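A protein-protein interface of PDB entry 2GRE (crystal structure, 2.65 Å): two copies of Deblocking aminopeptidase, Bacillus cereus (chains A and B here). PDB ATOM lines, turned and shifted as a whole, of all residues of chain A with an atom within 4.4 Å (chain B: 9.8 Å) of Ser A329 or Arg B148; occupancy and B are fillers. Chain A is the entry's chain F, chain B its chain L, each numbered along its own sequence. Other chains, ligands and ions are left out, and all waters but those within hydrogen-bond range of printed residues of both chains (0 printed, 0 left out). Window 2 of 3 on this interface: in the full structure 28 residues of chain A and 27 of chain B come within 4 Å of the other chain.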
ATOM      1  N   TYR A 179      15.980   2.320   8.017  1.00  0.00           N
ATOM      2  CA  TYR A 179      14.518   2.501   8.096  1.00  0.00           C
ATOM      3  C   TYR A 179      14.131   3.938   7.767  1.00  0.00           C
ATOM      4  O   TYR A 179      14.884   4.868   8.112  1.00  0.00           O
ATOM      5  CB  TYR A 179      13.994   2.182   9.513  1.00  0.00           C
ATOM      6  CG  TYR A 179      14.193   0.761   9.974  1.00  0.00           C
ATOM      7  CD1 TYR A 179      15.255   0.413  10.817  1.00  0.00           C
ATOM      8  CD2 TYR A 179      13.306  -0.233   9.600  1.00  0.00           C
ATOM      9  CE1 TYR A 179      15.422  -0.913  11.260  1.00  0.00           C
ATOM     10  CE2 TYR A 179      13.459  -1.556  10.038  1.00  0.00           C
ATOM     11  CZ  TYR A 179      14.513  -1.888  10.849  1.00  0.00           C
ATOM     12  OH  TYR A 179      14.642  -3.200  11.244  1.00  0.00           O
ATOM     13  N   TYR A 254      10.192  -5.654   5.036  1.00  0.00           N
ATOM     14  CA  TYR A 254      11.402  -5.961   4.281  1.00  0.00           C
ATOM     15  C   TYR A 254      11.119  -6.664   2.997  1.00  0.00           C
ATOM     16  O   TYR A 254      11.994  -7.386   2.498  1.00  0.00           O
ATOM     17  CB  TYR A 254      12.280  -6.907   5.086  1.00  0.00           C
ATOM     18  CG  TYR A 254      12.398  -6.460   6.490  1.00  0.00           C
ATOM     19  CD1 TYR A 254      11.587  -7.008   7.484  1.00  0.00           C
ATOM     20  CD2 TYR A 254      13.274  -5.434   6.831  1.00  0.00           C
ATOM     21  CE1 TYR A 254      11.684  -6.581   8.805  1.00  0.00           C
ATOM     22  CE2 TYR A 254      13.374  -4.990   8.141  1.00  0.00           C
ATOM     23  CZ  TYR A 254      12.567  -5.558   9.116  1.00  0.00           C
ATOM     24  OH  TYR A 254      12.664  -5.104  10.394  1.00  0.00           O
ATOM     25  N   HIS A 327      11.292  -0.446   5.652  1.00  0.00           N
ATOM     26  CA  HIS A 327      12.722  -0.591   5.536  1.00  0.00           C
ATOM     27  C   HIS A 327      13.168  -0.513   4.094  1.00  0.00           C
ATOM     28  O   HIS A 327      12.485  -1.010   3.196  1.00  0.00           O
ATOM     29  CB  HIS A 327      13.173  -1.888   6.197  1.00  0.00           C
ATOM     30  CG  HIS A 327      14.650  -2.015   6.331  1.00  0.00           C
ATOM     31  ND1 HIS A 327      15.411  -2.761   5.457  1.00  0.00           N
ATOM     32  CD2 HIS A 327      15.510  -1.510   7.252  1.00  0.00           C
ATOM     33  CE1 HIS A 327      16.681  -2.709   5.832  1.00  0.00           C
ATOM     34  NE2 HIS A 327      16.770  -1.955   6.918  1.00  0.00           N
ATOM     35  N   GLU A 328      14.332   0.087   3.882  1.00  0.00           N
ATOM     36  CA  GLU A 328      14.857   0.249   2.552  1.00  0.00           C
ATOM     37  C   GLU A 328      14.748  -1.025   1.683  1.00  0.00           C
ATOM     38  O   GLU A 328      14.519  -0.918   0.466  1.00  0.00           O
ATOM     39  CB  GLU A 328      16.296   0.803   2.595  1.00  0.00           C
ATOM     40  CG  GLU A 328      17.437  -0.227   2.823  1.00  0.00           C
ATOM     41  CD  GLU A 328      18.841   0.383   2.660  1.00  0.00           C
ATOM     42  OE1 GLU A 328      19.120   1.044   1.610  1.00  0.00           O
ATOM     43  OE2 GLU A 328      19.659   0.204   3.603  1.00  0.00           O
ATOM     44  N   SER A 329      14.881  -2.207   2.285  1.00  0.00           N
ATOM     45  CA  SER A 329      14.817  -3.433   1.482  1.00  0.00           C
ATOM     46  C   SER A 329      13.442  -3.598   0.856  1.00  0.00           C
ATOM     47  O   SER A 329      13.323  -4.083  -0.281  1.00  0.00           O
ATOM     48  CB  SER A 329      15.207  -4.685   2.265  1.00  0.00           C
ATOM     49  OG  SER A 329      14.629  -4.645   3.553  1.00  0.00           O
ATOM     50  N   SER A 330      12.415  -3.168   1.591  1.00  0.00           N
ATOM     51  CA  SER A 330      11.058  -3.224   1.077  1.00  0.00           C
ATOM     52  C   SER A 330      10.877  -2.347  -0.166  1.00  0.00           C
ATOM     53  O   SER A 330      10.288  -2.776  -1.166  1.00  0.00           O
ATOM     54  CB  SER A 330      10.084  -2.759   2.124  1.00  0.00           C
ATOM     55  OG  SER A 330       8.771  -2.936   1.635  1.00  0.00           O
ATOM     56  N   ILE A 331      11.360  -1.106  -0.054  1.00  0.00           N
ATOM     57  CA  ILE A 331      11.390  -0.148  -1.139  1.00  0.00           C
ATOM     58  C   ILE A 331      12.149  -0.763  -2.329  1.00  0.00           C
ATOM     59  O   ILE A 331      11.623  -0.776  -3.455  1.00  0.00           O
ATOM     60  CB  ILE A 331      12.166   1.158  -0.731  1.00  0.00           C
ATOM     61  CG1 ILE A 331      11.732   1.771   0.629  1.00  0.00           C
ATOM     62  CG2 ILE A 331      12.192   2.160  -1.865  1.00  0.00           C
ATOM     63  CD1 ILE A 331      10.445   2.309   0.655  1.00  0.00           C
ATOM     64  N   ALA A 332      13.372  -1.264  -2.085  1.00  0.00           N
ATOM     65  CA  ALA A 332      14.153  -1.916  -3.150  1.00  0.00           C
ATOM     66  C   ALA A 332      13.343  -2.974  -3.899  1.00  0.00           C
ATOM     67  O   ALA A 332      13.201  -2.931  -5.139  1.00  0.00           O
ATOM     68  CB  ALA A 332      15.418  -2.491  -2.614  1.00  0.00           C
ATOM     69  N   HIS A 333      12.762  -3.877  -3.127  1.00  0.00           N
ATOM     70  CA  HIS A 333      12.016  -4.989  -3.670  1.00  0.00           C
ATOM     71  C   HIS A 333      10.802  -4.470  -4.394  1.00  0.00           C
ATOM     72  O   HIS A 333      10.505  -4.887  -5.507  1.00  0.00           O
ATOM     73  CB  HIS A 333      11.609  -5.970  -2.554  1.00  0.00           C
ATOM     74  CG  HIS A 333      12.746  -6.824  -2.061  1.00  0.00           C
ATOM     75  ND1 HIS A 333      13.584  -7.506  -2.908  1.00  0.00           N
ATOM     76  CD2 HIS A 333      13.178  -7.102  -0.818  1.00  0.00           C
ATOM     77  CE1 HIS A 333      14.488  -8.169  -2.225  1.00  0.00           C
ATOM     78  NE2 HIS A 333      14.270  -7.932  -0.950  1.00  0.00           N
ATOM     79  N   ASP B  83       9.270 -11.717  20.094  1.00  0.00           N
ATOM     80  CA  ASP B  83       9.115 -11.115  18.762  1.00  0.00           C
ATOM     81  C   ASP B  83      10.253 -10.106  18.441  1.00  0.00           C
ATOM     82  O   ASP B  83      10.507  -9.761  17.286  1.00  0.00           O
ATOM     83  CB  ASP B  83       7.713 -10.461  18.618  1.00  0.00           C
ATOM     84  CG  ASP B  83       7.564  -9.126  19.428  1.00  0.00           C
ATOM     85  OD1 ASP B  83       6.963  -8.175  18.875  1.00  0.00           O
ATOM     86  OD2 ASP B  83       8.026  -9.024  20.598  1.00  0.00           O
ATOM     87  N   GLY B  84      10.936  -9.642  19.479  1.00  0.00           N
ATOM     88  CA  GLY B  84      11.967  -8.626  19.320  1.00  0.00           C
ATOM     89  C   GLY B  84      11.708  -7.337  20.089  1.00  0.00           C
ATOM     90  O   GLY B  84      12.645  -6.574  20.359  1.00  0.00           O
ATOM     91  N   TYR B 114      20.370   3.462  21.140  1.00  0.00           N
ATOM     92  CA  TYR B 114      19.481   3.062  20.032  1.00  0.00           C
ATOM     93  C   TYR B 114      18.184   3.845  19.943  1.00  0.00           C
ATOM     94  O   TYR B 114      17.664   4.339  20.961  1.00  0.00           O
ATOM     95  CB  TYR B 114      19.144   1.572  20.092  1.00  0.00           C
ATOM     96  CG  TYR B 114      20.349   0.677  19.989  1.00  0.00           C
ATOM     97  CD1 TYR B 114      20.973   0.220  21.146  1.00  0.00           C
ATOM     98  CD2 TYR B 114      20.891   0.307  18.749  1.00  0.00           C
ATOM     99  CE1 TYR B 114      22.074  -0.620  21.096  1.00  0.00           C
ATOM    100  CE2 TYR B 114      22.018  -0.541  18.680  1.00  0.00           C
ATOM    101  CZ  TYR B 114      22.602  -1.004  19.883  1.00  0.00           C
ATOM    102  OH  TYR B 114      23.701  -1.834  19.920  1.00  0.00           O
ATOM    103  N   THR B 115      17.646   3.942  18.731  1.00  0.00           N
ATOM    104  CA  THR B 115      16.394   4.646  18.560  1.00  0.00           C
ATOM    105  C   THR B 115      15.254   3.651  18.388  1.00  0.00           C
ATOM    106  O   THR B 115      15.470   2.510  17.970  1.00  0.00           O
ATOM    107  CB  THR B 115      16.453   5.687  17.420  1.00  0.00           C
ATOM    108  OG1 THR B 115      16.560   5.015  16.156  1.00  0.00           O
ATOM    109  CG2 THR B 115      17.647   6.664  17.615  1.00  0.00           C
ATOM    110  N   ARG B 144       9.398  -0.547  19.470  1.00  0.00           N
ATOM    111  CA  ARG B 144       9.852  -1.114  18.200  1.00  0.00           C
ATOM    112  C   ARG B 144      11.230  -0.514  17.929  1.00  0.00           C
ATOM    113  O   ARG B 144      11.357   0.710  17.723  1.00  0.00           O
ATOM    114  CB  ARG B 144       8.856  -0.724  17.122  1.00  0.00           C
ATOM    115  CG  ARG B 144       9.182  -1.108  15.706  1.00  0.00           C
ATOM    116  CD  ARG B 144       9.028   0.156  14.865  1.00  0.00           C
ATOM    117  NE  ARG B 144       7.692   0.484  14.342  1.00  0.00           N
ATOM    118  CZ  ARG B 144       7.247   1.735  14.158  1.00  0.00           C
ATOM    119  NH1 ARG B 144       7.993   2.772  14.502  1.00  0.00           N
ATOM    120  NH2 ARG B 144       6.048   1.956  13.636  1.00  0.00           N
ATOM    121  N   ILE B 145      12.268  -1.348  17.979  1.00  0.00           N
ATOM    122  CA  ILE B 145      13.629  -0.841  17.826  1.00  0.00           C
ATOM    123  C   ILE B 145      13.955  -0.630  16.371  1.00  0.00           C
ATOM    124  O   ILE B 145      13.453  -1.352  15.515  1.00  0.00           O
ATOM    125  CB  ILE B 145      14.654  -1.807  18.361  1.00  0.00           C
ATOM    126  CG1 ILE B 145      14.083  -2.613  19.527  1.00  0.00           C
ATOM    127  CG2 ILE B 145      15.901  -1.068  18.785  1.00  0.00           C
ATOM    128  CD1 ILE B 145      15.125  -3.432  20.230  1.00  0.00           C
ATOM    129  N   ASP B 146      14.793   0.360  16.089  1.00  0.00           N
ATOM    130  CA  ASP B 146      15.190   0.667  14.731  1.00  0.00           C
ATOM    131  C   ASP B 146      16.402  -0.189  14.352  1.00  0.00           C
ATOM    132  O   ASP B 146      17.447   0.322  13.958  1.00  0.00           O
ATOM    133  CB  ASP B 146      15.460   2.178  14.557  1.00  0.00           C
ATOM    134  CG  ASP B 146      14.217   3.048  14.835  1.00  0.00           C
ATOM    135  OD1 ASP B 146      13.100   2.673  14.444  1.00  0.00           O
ATOM    136  OD2 ASP B 146      14.335   4.118  15.465  1.00  0.00           O
ATOM    137  N   GLU B 147      16.264  -1.502  14.461  1.00  0.00           N
ATOM    138  CA  GLU B 147      17.333  -2.413  14.079  1.00  0.00           C
ATOM    139  C   GLU B 147      16.705  -3.658  13.483  1.00  0.00           C
ATOM    140  O   GLU B 147      15.646  -4.063  13.957  1.00  0.00           O
ATOM    141  CB  GLU B 147      18.202  -2.794  15.292  1.00  0.00           C
ATOM    142  CG  GLU B 147      19.034  -1.638  15.912  1.00  0.00           C
ATOM    143  CD  GLU B 147      20.020  -0.976  14.939  1.00  0.00           C
ATOM    144  OE1 GLU B 147      20.523   0.122  15.267  1.00  0.00           O
ATOM    145  OE2 GLU B 147      20.298  -1.545  13.851  1.00  0.00           O
ATOM    146  N   ARG B 148      17.326  -4.255  12.455  1.00  0.00           N
ATOM    147  CA  ARG B 148      16.842  -5.524  11.926  1.00  0.00           C
ATOM    148  C   ARG B 148      17.087  -6.679  12.910  1.00  0.00           C
ATOM    149  O   ARG B 148      17.866  -7.580  12.627  1.00  0.00           O
ATOM    150  CB  ARG B 148      17.494  -5.841  10.602  1.00  0.00           C
ATOM    151  CG  ARG B 148      17.453  -4.707   9.617  1.00  0.00           C
ATOM    152  CD  ARG B 148      18.056  -5.125   8.314  1.00  0.00           C
ATOM    153  NE  ARG B 148      17.170  -6.063   7.617  1.00  0.00           N
ATOM    154  CZ  ARG B 148      17.369  -6.489   6.365  1.00  0.00           C
ATOM    155  NH1 ARG B 148      18.427  -6.056   5.699  1.00  0.00           N
ATOM    156  NH2 ARG B 148      16.515  -7.332   5.772  1.00  0.00           N
ATOM    157  N   VAL B 149      16.419  -6.634  14.065  1.00  0.00           N
ATOM    158  CA  VAL B 149      16.420  -7.742  15.011  1.00  0.00           C
ATOM    159  C   VAL B 149      15.034  -8.357  15.156  1.00  0.00           C
ATOM    160  O   VAL B 149      14.046  -7.648  15.355  1.00  0.00           O
ATOM    161  CB  VAL B 149      16.941  -7.322  16.417  1.00  0.00           C
ATOM    162  CG1 VAL B 149      18.455  -7.160  16.387  1.00  0.00           C
ATOM    163  CG2 VAL B 149      16.250  -6.056  16.906  1.00  0.00           C
ATOM    164  N   PHE B 150      14.962  -9.679  15.076  1.00  0.00           N
ATOM    165  CA  PHE B 150      13.667 -10.355  15.143  1.00  0.00           C
ATOM    166  C   PHE B 150      13.530 -11.331  16.282  1.00  0.00           C
ATOM    167  O   PHE B 150      12.754 -12.276  16.182  1.00  0.00           O
ATOM    168  CB  PHE B 150      13.391 -11.063  13.828  1.00  0.00           C
ATOM    169  CG  PHE B 150      13.678 -10.218  12.655  1.00  0.00           C
ATOM    170  CD1 PHE B 150      14.561 -10.644  11.679  1.00  0.00           C
ATOM    171  CD2 PHE B 150      13.096  -8.960  12.544  1.00  0.00           C
ATOM    172  CE1 PHE B 150      14.838  -9.845  10.592  1.00  0.00           C
ATOM    173  CE2 PHE B 150      13.369  -8.155  11.473  1.00  0.00           C
ATOM    174  CZ  PHE B 150      14.245  -8.597  10.495  1.00  0.00           C
ATOM    175  N   SER B 151      14.290 -11.113  17.357  1.00  0.00           N
ATOM    176  CA  SER B 151      14.185 -11.967  18.536  1.00  0.00           C
ATOM    177  C   SER B 151      14.921 -11.401  19.725  1.00  0.00           C
ATOM    178  O   SER B 151      15.759 -10.506  19.591  1.00  0.00           O
ATOM    179  CB  SER B 151      14.703 -13.375  18.239  1.00  0.00           C
ATOM    180  OG  SER B 151      16.120 -13.403  18.195  1.00  0.00           O
ATOM    181  N   ASP B 153      17.362 -12.893  21.506  1.00  0.00           N
ATOM    182  CA  ASP B 153      18.831 -13.056  21.480  1.00  0.00           C
ATOM    183  C   ASP B 153      19.484 -11.966  20.657  1.00  0.00           C
ATOM    184  O   ASP B 153      20.412 -11.296  21.129  1.00  0.00           O
ATOM    185  CB  ASP B 153      19.295 -14.432  20.974  1.00  0.00           C
ATOM    186  CG  ASP B 153      18.694 -15.590  21.760  1.00  0.00           C
ATOM    187  OD1 ASP B 153      17.459 -15.752  21.660  1.00  0.00           O
ATOM    188  OD2 ASP B 153      19.429 -16.348  22.443  1.00  0.00           O
ATOM    189  N   GLU B 154      18.980 -11.775  19.438  1.00  0.00           N
ATOM    190  CA  GLU B 154      19.457 -10.707  18.558  1.00  0.00           C
ATOM    191  C   GLU B 154      19.409  -9.332  19.225  1.00  0.00           C
ATOM    192  O   GLU B 154      20.287  -8.502  18.992  1.00  0.00           O
ATOM    193  CB  GLU B 154      18.722 -10.725  17.215  1.00  0.00           C
ATOM    194  CG  GLU B 154      19.046 -11.997  16.385  1.00  0.00           C
ATOM    195  CD  GLU B 154      18.157 -12.237  15.149  1.00  0.00           C
ATOM    196  OE1 GLU B 154      18.525 -13.110  14.343  1.00  0.00           O
ATOM    197  OE2 GLU B 154      17.112 -11.578  14.962  1.00  0.00           O
ATOM    198  N   VAL B 155      18.420  -9.104  20.085  1.00  0.00           N
ATOM    199  CA  VAL B 155      18.358  -7.826  20.795  1.00  0.00           C
ATOM    200  C   VAL B 155      19.475  -7.785  21.852  1.00  0.00           C
ATOM    201  O   VAL B 155      20.215  -6.789  21.956  1.00  0.00           O
ATOM    202  CB  VAL B 155      16.941  -7.532  21.411  1.00  0.00           C
ATOM    203  CG1 VAL B 155      16.983  -6.437  22.478  1.00  0.00           C
ATOM    204  CG2 VAL B 155      15.938  -7.167  20.342  1.00  0.00           C
ATOM    205  N   GLU B 157      22.211  -9.197  21.678  1.00  0.00           N
ATOM    206  CA  GLU B 157      23.466  -9.000  20.935  1.00  0.00           C
ATOM    207  C   GLU B 157      23.799  -7.534  20.651  1.00  0.00           C
ATOM    208  O   GLU B 157      24.947  -7.177  20.463  1.00  0.00           O
ATOM    209  CB  GLU B 157      23.474  -9.832  19.652  1.00  0.00           C
ATOM    210  CG  GLU B 157      23.387 -11.339  19.927  1.00  0.00           C
ATOM    211  CD  GLU B 157      23.404 -12.202  18.668  1.00  0.00           C
ATOM    212  OE1 GLU B 157      24.132 -13.231  18.698  1.00  0.00           O
ATOM    213  OE2 GLU B 157      22.703 -11.863  17.667  1.00  0.00           O
ATOM    214  N   LEU B 158      22.775  -6.694  20.632  1.00  0.00           N
ATOM    215  CA  LEU B 158      22.941  -5.252  20.535  1.00  0.00           C
ATOM    216  C   LEU B 158      23.541  -4.628  21.813  1.00  0.00           C
ATOM    217  O   LEU B 158      24.109  -3.531  21.757  1.00  0.00           O
ATOM    218  CB  LEU B 158      21.590  -4.603  20.259  1.00  0.00           C
ATOM    219  CG  LEU B 158      21.153  -4.090  18.885  1.00  0.00           C
ATOM    220  CD1 LEU B 158      21.804  -4.727  17.657  1.00  0.00           C
ATOM    221  CD2 LEU B 158      19.638  -4.198  18.817  1.00  0.00           C
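OH of Tyr A179 lies within hydrogen-bond range of O of Glu B147 (3.0 Å). The side-chain hydroxyl (OH) of Tyr A179 is in hydrogen-bond range of the backbone NH (N) of Arg B148 (3.1 Å).
OH of Tyr A254 is in hydrogen-bond range of OH of Tyr A179. ND1 of His A327 sits at hydrogen-bond distance from OG of Ser A329, at 2.8 Å. The side-chain carboxylate (OD2) of Asp B146 sits at hydrogen-bond distance from the side-chain hydroxyl (OG1) of Thr B115. N of Phe B150 sits at hydrogen-bond distance from OE2 of Glu B154 (2.9 Å).
Among the printed residues, pairs that only touch across the chains: Tyr A179 with Asp B146 (3.3 Å), Tyr A254 with Arg B148 (3.9 Å), Tyr A254 with Phe B150 (3.3 Å), His A327 with Arg B148 (3.7 Å) and Ser A329 with Arg B148 (3.96 Å).
Of the printed residues of chain B, Ser A329 touches Arg B148 (3.96 Å). Of chain A, only Tyr A179, Tyr A254, His A327 and Ser A329 come within 4 Å of Arg B148. Printed residues of chain B within 4 Å of Tyr A254: Arg B148 and Phe B150. Of chain B, only Arg B148 (3.7 Å) comes within 4 Å of His A327. No residue of chain B comes within 4 Å of Ser A330. No residue of chain B comes within 4 Å of Ala A332. Printed residues of chain B within 4 Å of Tyr A179: Asp B146, Glu B147 and Arg B148. Printed residues of chain A within 4 Å of Asp B146: Tyr A179 (3.3 Å). Of the printed residues of chain A, Phe B150 touches Tyr A254 (3.3 Å). Val B155 touches none of the printed residues of chain A. The nearest printed residue of chain A that does not touch Phe B150 is Tyr A179 (5.1 Å).
Hydrophobic or aromatic side chains of chain B that line the printed part of chain A: Phe B150. Among the printed residues, 7 pairs touch across the chains.
No position is printed for both chains.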
